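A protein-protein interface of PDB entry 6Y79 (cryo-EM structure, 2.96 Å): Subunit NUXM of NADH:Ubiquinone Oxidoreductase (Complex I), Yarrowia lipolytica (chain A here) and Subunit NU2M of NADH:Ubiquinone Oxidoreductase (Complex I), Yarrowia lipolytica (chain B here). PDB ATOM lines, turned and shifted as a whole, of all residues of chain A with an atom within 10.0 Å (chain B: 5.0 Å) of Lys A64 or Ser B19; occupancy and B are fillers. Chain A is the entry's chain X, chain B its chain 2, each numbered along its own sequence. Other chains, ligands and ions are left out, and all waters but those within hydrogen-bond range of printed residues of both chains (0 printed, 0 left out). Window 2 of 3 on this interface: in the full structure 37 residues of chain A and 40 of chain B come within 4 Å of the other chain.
The backbone NH (N) of Val A63 sits at hydrogen-bond distance from the side-chain carboxylate (OE2) of Glu A58 (2.9 Å).
Asp A61 touches Asn B86.
Pro A62 touches Asn B86 (O to ND2, 3.9 Å).
Ser B19 touches Lys A64 (O to NZ, 3.5 Å).
Gly A65 touches Asn B89.
Phe A74 touches Asp B20 (CZ to CB, 3.8 Å).
O of Val A63 lies within hydrogen-bond range of ND2 of Asn B86 (2.6 Å).
Of the printed residues of chain B, Asp A61 touches Asn B86 (3.97 Å).
Printed residues of chain B within 4 Å of Pro A62: Asn B86 (3.9 Å).
Of the printed residues of chain B, Gly A65 touches Asn B89 (3.6 Å).
No residue of chain A comes within 4 Å of Leu B18.
Ser B19 touches one residue of chain A.
Asp B20 touches just one residue of chain A: Phe A74 (3.8 Å).
Of the printed residues of chain A, Asn B86 touches Asp A61 (3.97 Å), Pro A62 (3.9 Å) and Val A63 (2.6 Å).
The nearest residue of chain B that does not touch Lys A64 is Lys B94 (4.7 Å).
The nearest residue of chain A that does not touch Ser B19 is Val A63 (5.7 Å).
Of the 14 printed residues of chain A, 6 touch a printed residue of chain B.
Hydrophobic or aromatic side chains of chain A that line the printed part of chain B: Phe A74.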
ATOM      1  N   ALA A  57       6.385  14.901  -8.386  1.00  0.00           N
ATOM      2  CA  ALA A  57       6.427  15.072  -9.831  1.00  0.00           C
ATOM      3  C   ALA A  57       5.280  14.368 -10.539  1.00  0.00           C
ATOM      4  O   ALA A  57       4.968  14.719 -11.678  1.00  0.00           O
ATOM      5  CB  ALA A  57       7.762  14.571 -10.370  1.00  0.00           C
ATOM      6  N   GLU A  58       4.653  13.381  -9.900  1.00  0.00           N
ATOM      7  CA  GLU A  58       3.402  12.849 -10.426  1.00  0.00           C
ATOM      8  C   GLU A  58       2.235  13.785 -10.143  1.00  0.00           C
ATOM      9  O   GLU A  58       1.339  13.938 -10.979  1.00  0.00           O
ATOM     10  CB  GLU A  58       3.120  11.474  -9.831  1.00  0.00           C
ATOM     11  CG  GLU A  58       1.921  10.782 -10.435  1.00  0.00           C
ATOM     12  CD  GLU A  58       2.236  10.181 -11.779  1.00  0.00           C
ATOM     13  OE1 GLU A  58       3.434   9.974 -12.057  1.00  0.00           O
ATOM     14  OE2 GLU A  58       1.296   9.914 -12.556  1.00  0.00           O
ATOM     15  N   ASP A  61       2.478  16.735 -12.856  1.00  0.00           N
ATOM     16  CA  ASP A  61       2.059  16.254 -14.172  1.00  0.00           C
ATOM     17  C   ASP A  61       1.868  14.744 -14.126  1.00  0.00           C
ATOM     18  O   ASP A  61       2.862  14.007 -14.098  1.00  0.00           O
ATOM     19  CB  ASP A  61       3.103  16.594 -15.244  1.00  0.00           C
ATOM     20  CG  ASP A  61       2.537  16.649 -16.654  1.00  0.00           C
ATOM     21  OD1 ASP A  61       1.915  17.671 -17.009  1.00  0.00           O
ATOM     22  OD2 ASP A  61       2.738  15.686 -17.426  1.00  0.00           O
ATOM     23  N   PRO A  62       0.638  14.238 -14.092  1.00  0.00           N
ATOM     24  CA  PRO A  62       0.444  12.785 -14.059  1.00  0.00           C
ATOM     25  C   PRO A  62       0.759  12.137 -15.398  1.00  0.00           C
ATOM     26  O   PRO A  62       0.703  12.765 -16.454  1.00  0.00           O
ATOM     27  CB  PRO A  62      -1.036  12.632 -13.701  1.00  0.00           C
ATOM     28  CG  PRO A  62      -1.404  13.915 -13.056  1.00  0.00           C
ATOM     29  CD  PRO A  62      -0.607  14.951 -13.775  1.00  0.00           C
ATOM     30  N   VAL A  63       1.084  10.844 -15.333  1.00  0.00           N
ATOM     31  CA  VAL A  63       1.592  10.135 -16.504  1.00  0.00           C
ATOM     32  C   VAL A  63       0.478   9.856 -17.503  1.00  0.00           C
ATOM     33  O   VAL A  63       0.568  10.241 -18.673  1.00  0.00           O
ATOM     34  CB  VAL A  63       2.300   8.835 -16.081  1.00  0.00           C
ATOM     35  CG1 VAL A  63       2.723   8.054 -17.303  1.00  0.00           C
ATOM     36  CG2 VAL A  63       3.502   9.139 -15.236  1.00  0.00           C
ATOM     37  N   LYS A  64      -0.581   9.178 -17.071  1.00  0.00           N
ATOM     38  CA  LYS A  64      -1.667   8.794 -17.963  1.00  0.00           C
ATOM     39  C   LYS A  64      -2.884   9.701 -17.844  1.00  0.00           C
ATOM     40  O   LYS A  64      -4.003   9.260 -18.118  1.00  0.00           O
ATOM     41  CB  LYS A  64      -2.075   7.342 -17.717  1.00  0.00           C
ATOM     42  CG  LYS A  64      -0.914   6.381 -17.707  1.00  0.00           C
ATOM     43  CD  LYS A  64      -0.596   5.897 -19.112  1.00  0.00           C
ATOM     44  CE  LYS A  64       0.831   5.380 -19.201  1.00  0.00           C
ATOM     45  NZ  LYS A  64       0.996   4.075 -18.509  1.00  0.00           N
ATOM     46  N   GLY A  65      -2.694  10.951 -17.450  1.00  0.00           N
ATOM     47  CA  GLY A  65      -3.763  11.932 -17.472  1.00  0.00           C
ATOM     48  C   GLY A  65      -4.415  12.315 -16.163  1.00  0.00           C
ATOM     49  O   GLY A  65      -4.605  13.505 -15.912  1.00  0.00           O
ATOM     50  N   LYS A  66      -4.774  11.348 -15.322  1.00  0.00           N
ATOM     51  CA  LYS A  66      -5.289  11.673 -14.000  1.00  0.00           C
ATOM     52  C   LYS A  66      -4.457  10.993 -12.918  1.00  0.00           C
ATOM     53  O   LYS A  66      -3.859   9.936 -13.130  1.00  0.00           O
ATOM     54  CB  LYS A  66      -6.771  11.298 -13.849  1.00  0.00           C
ATOM     55  CG  LYS A  66      -7.116   9.832 -13.750  1.00  0.00           C
ATOM     56  CD  LYS A  66      -8.615   9.707 -13.533  1.00  0.00           C
ATOM     57  CE  LYS A  66      -9.005  10.245 -12.164  1.00  0.00           C
ATOM     58  NZ  LYS A  66      -8.476   9.394 -11.066  1.00  0.00           N
ATOM     59  N   PHE A  67      -4.446  11.615 -11.748  1.00  0.00           N
ATOM     60  CA  PHE A  67      -3.438  11.356 -10.730  1.00  0.00           C
ATOM     61  C   PHE A  67      -3.695  10.035 -10.014  1.00  0.00           C
ATOM     62  O   PHE A  67      -4.788   9.800  -9.491  1.00  0.00           O
ATOM     63  CB  PHE A  67      -3.419  12.505  -9.727  1.00  0.00           C
ATOM     64  CG  PHE A  67      -2.491  12.290  -8.582  1.00  0.00           C
ATOM     65  CD1 PHE A  67      -1.125  12.360  -8.767  1.00  0.00           C
ATOM     66  CD2 PHE A  67      -2.983  12.031  -7.319  1.00  0.00           C
ATOM     67  CE1 PHE A  67      -0.266  12.167  -7.709  1.00  0.00           C
ATOM     68  CE2 PHE A  67      -2.131  11.840  -6.260  1.00  0.00           C
ATOM     69  CZ  PHE A  67      -0.769  11.911  -6.455  1.00  0.00           C
ATOM     70  N   ALA A  68      -2.680   9.180  -9.990  1.00  0.00           N
ATOM     71  CA  ALA A  68      -2.609   8.056  -9.078  1.00  0.00           C
ATOM     72  C   ALA A  68      -1.299   8.159  -8.316  1.00  0.00           C
ATOM     73  O   ALA A  68      -0.392   8.900  -8.700  1.00  0.00           O
ATOM     74  CB  ALA A  68      -2.704   6.715  -9.816  1.00  0.00           C
ATOM     75  N   ARG A  69      -1.213   7.435  -7.216  1.00  0.00           N
ATOM     76  CA  ARG A  69       0.077   7.268  -6.582  1.00  0.00           C
ATOM     77  C   ARG A  69       0.949   6.389  -7.473  1.00  0.00           C
ATOM     78  O   ARG A  69       0.435   5.517  -8.179  1.00  0.00           O
ATOM     79  CB  ARG A  69      -0.088   6.627  -5.204  1.00  0.00           C
ATOM     80  CG  ARG A  69       1.165   6.620  -4.344  1.00  0.00           C
ATOM     81  CD  ARG A  69       0.906   6.184  -2.914  1.00  0.00           C
ATOM     82  NE  ARG A  69       2.154   6.032  -2.169  1.00  0.00           N
ATOM     83  CZ  ARG A  69       2.820   7.037  -1.605  1.00  0.00           C
ATOM     84  NH1 ARG A  69       2.361   8.276  -1.697  1.00  0.00           N
ATOM     85  NH2 ARG A  69       3.945   6.804  -0.945  1.00  0.00           N
ATOM     86  N   SER A  71       3.507   3.295  -8.175  1.00  0.00           N
ATOM     87  CA  SER A  71       3.501   1.940  -7.650  1.00  0.00           C
ATOM     88  C   SER A  71       4.535   1.788  -6.538  1.00  0.00           C
ATOM     89  O   SER A  71       5.449   2.597  -6.379  1.00  0.00           O
ATOM     90  CB  SER A  71       3.789   0.935  -8.764  1.00  0.00           C
ATOM     91  OG  SER A  71       2.781   0.956  -9.756  1.00  0.00           O
ATOM     92  N   LYS A  73       6.605  -0.616  -6.504  1.00  0.00           N
ATOM     93  CA  LYS A  73       7.819  -1.051  -7.185  1.00  0.00           C
ATOM     94  C   LYS A  73       8.706   0.124  -7.564  1.00  0.00           C
ATOM     95  O   LYS A  73       9.924  -0.037  -7.673  1.00  0.00           O
ATOM     96  CB  LYS A  73       7.470  -1.873  -8.430  1.00  0.00           C
ATOM     97  CG  LYS A  73       6.832  -1.096  -9.576  1.00  0.00           C
ATOM     98  CD  LYS A  73       6.764  -1.911 -10.849  1.00  0.00           C
ATOM     99  CE  LYS A  73       8.146  -2.235 -11.380  1.00  0.00           C
ATOM    100  NZ  LYS A  73       8.138  -3.479 -12.200  1.00  0.00           N
ATOM    101  N   PHE A  74       8.125   1.305  -7.759  1.00  0.00           N
ATOM    102  CA  PHE A  74       8.904   2.506  -7.995  1.00  0.00           C
ATOM    103  C   PHE A  74       9.364   3.145  -6.699  1.00  0.00           C
ATOM    104  O   PHE A  74      10.468   3.694  -6.651  1.00  0.00           O
ATOM    105  CB  PHE A  74       8.088   3.523  -8.794  1.00  0.00           C
ATOM    106  CG  PHE A  74       7.835   3.122 -10.217  1.00  0.00           C
ATOM    107  CD1 PHE A  74       8.694   2.274 -10.881  1.00  0.00           C
ATOM    108  CD2 PHE A  74       6.729   3.597 -10.890  1.00  0.00           C
ATOM    109  CE1 PHE A  74       8.456   1.906 -12.194  1.00  0.00           C
ATOM    110  CE2 PHE A  74       6.489   3.228 -12.200  1.00  0.00           C
ATOM    111  CZ  PHE A  74       7.359   2.382 -12.849  1.00  0.00           C
ATOM    112  N   LYS B  17       7.922  -3.267 -17.682  1.00  0.00           N
ATOM    113  CA  LYS B  17       7.262  -3.393 -18.963  1.00  0.00           C
ATOM    114  C   LYS B  17       7.428  -2.087 -19.725  1.00  0.00           C
ATOM    115  O   LYS B  17       8.013  -1.119 -19.233  1.00  0.00           O
ATOM    116  CB  LYS B  17       5.795  -3.752 -18.779  1.00  0.00           C
ATOM    117  CG  LYS B  17       5.554  -5.127 -18.191  1.00  0.00           C
ATOM    118  CD  LYS B  17       4.074  -5.421 -18.112  1.00  0.00           C
ATOM    119  CE  LYS B  17       3.403  -4.551 -17.058  1.00  0.00           C
ATOM    120  NZ  LYS B  17       3.829  -4.887 -15.671  1.00  0.00           N
ATOM    121  N   LEU B  18       6.913  -2.057 -20.950  1.00  0.00           N
ATOM    122  CA  LEU B  18       7.075  -0.869 -21.775  1.00  0.00           C
ATOM    123  C   LEU B  18       6.083   0.210 -21.366  1.00  0.00           C
ATOM    124  O   LEU B  18       6.211   1.366 -21.776  1.00  0.00           O
ATOM    125  CB  LEU B  18       6.924  -1.231 -23.249  1.00  0.00           C
ATOM    126  CG  LEU B  18       8.022  -1.914 -24.076  1.00  0.00           C
ATOM    127  CD1 LEU B  18       8.193  -3.358 -23.639  1.00  0.00           C
ATOM    128  CD2 LEU B  18       7.536  -1.871 -25.499  1.00  0.00           C
ATOM    129  N   SER B  19       5.087  -0.151 -20.560  1.00  0.00           N
ATOM    130  CA  SER B  19       4.156   0.805 -19.985  1.00  0.00           C
ATOM    131  C   SER B  19       4.825   1.714 -18.960  1.00  0.00           C
ATOM    132  O   SER B  19       4.286   2.779 -18.646  1.00  0.00           O
ATOM    133  CB  SER B  19       2.992   0.069 -19.322  1.00  0.00           C
ATOM    134  OG  SER B  19       2.376  -0.853 -20.216  1.00  0.00           O
ATOM    135  N   ASP B  20       5.988   1.324 -18.444  1.00  0.00           N
ATOM    136  CA  ASP B  20       6.618   1.979 -17.311  1.00  0.00           C
ATOM    137  C   ASP B  20       7.783   2.878 -17.693  1.00  0.00           C
ATOM    138  O   ASP B  20       8.245   3.627 -16.822  1.00  0.00           O
ATOM    139  CB  ASP B  20       7.086   0.919 -16.319  1.00  0.00           C
ATOM    140  CG  ASP B  20       5.928   0.163 -15.710  1.00  0.00           C
ATOM    141  OD1 ASP B  20       4.835   0.759 -15.601  1.00  0.00           O
ATOM    142  OD2 ASP B  20       6.094  -1.023 -15.353  1.00  0.00           O
ATOM    143  N   ASN B  21       8.210   2.838 -18.972  1.00  0.00           N
ATOM    144  CA  ASN B  21       9.420   3.514 -19.451  1.00  0.00           C
ATOM    145  C   ASN B  21       9.442   4.982 -19.078  1.00  0.00           C
ATOM    146  O   ASN B  21      10.411   5.453 -18.468  1.00  0.00           O
ATOM    147  CB  ASN B  21       9.534   3.402 -20.971  1.00  0.00           C
ATOM    148  CG  ASN B  21       9.850   2.012 -21.434  1.00  0.00           C
ATOM    149  OD1 ASN B  21      10.532   1.251 -20.750  1.00  0.00           O
ATOM    150  ND2 ASN B  21       9.377   1.674 -22.622  1.00  0.00           N
ATOM    151  N   ASN B  86       4.819  14.208 -20.479  1.00  0.00           N
ATOM    152  CA  ASN B  86       3.960  14.390 -21.631  1.00  0.00           C
ATOM    153  C   ASN B  86       3.858  15.863 -21.972  1.00  0.00           C
ATOM    154  O   ASN B  86       3.847  16.724 -21.091  1.00  0.00           O
ATOM    155  CB  ASN B  86       2.564  13.848 -21.347  1.00  0.00           C
ATOM    156  CG  ASN B  86       2.551  12.366 -21.134  1.00  0.00           C
ATOM    157  OD1 ASN B  86       3.072  11.611 -21.943  1.00  0.00           O
ATOM    158  ND2 ASN B  86       1.959  11.934 -20.033  1.00  0.00           N
ATOM    159  N   ASN B  89      -1.991  15.489 -23.017  1.00  0.00           N
ATOM    160  CA  ASN B  89      -2.645  14.191 -22.946  1.00  0.00           C
ATOM    161  C   ASN B  89      -3.640  14.066 -24.097  1.00  0.00           C
ATOM    162  O   ASN B  89      -4.856  14.074 -23.927  1.00  0.00           O
ATOM    163  CB  ASN B  89      -3.308  14.015 -21.591  1.00  0.00           C
ATOM    164  CG  ASN B  89      -2.305  13.983 -20.470  1.00  0.00           C
ATOM    165  OD1 ASN B  89      -1.279  13.317 -20.571  1.00  0.00           O
ATOM    166  ND2 ASN B  89      -2.585  14.711 -19.397  1.00  0.00           N
ATOM    167  N   LYS B  94       1.122  11.125 -27.734  1.00  0.00           N
ATOM    168  CA  LYS B  94       1.596   9.793 -27.383  1.00  0.00           C
ATOM    169  C   LYS B  94       2.178   9.064 -28.594  1.00  0.00           C
ATOM    170  O   LYS B  94       3.132   8.296 -28.451  1.00  0.00           O
ATOM    171  CB  LYS B  94       0.464   8.992 -26.742  1.00  0.00           C
ATOM    172  CG  LYS B  94      -0.024   9.569 -25.420  1.00  0.00           C
ATOM    173  CD  LYS B  94      -1.224   8.782 -24.892  1.00  0.00           C
ATOM    174  CE  LYS B  94      -1.921   9.494 -23.728  1.00  0.00           C
ATOM    175  NZ  LYS B  94      -1.037   9.656 -22.541  1.00  0.00           N
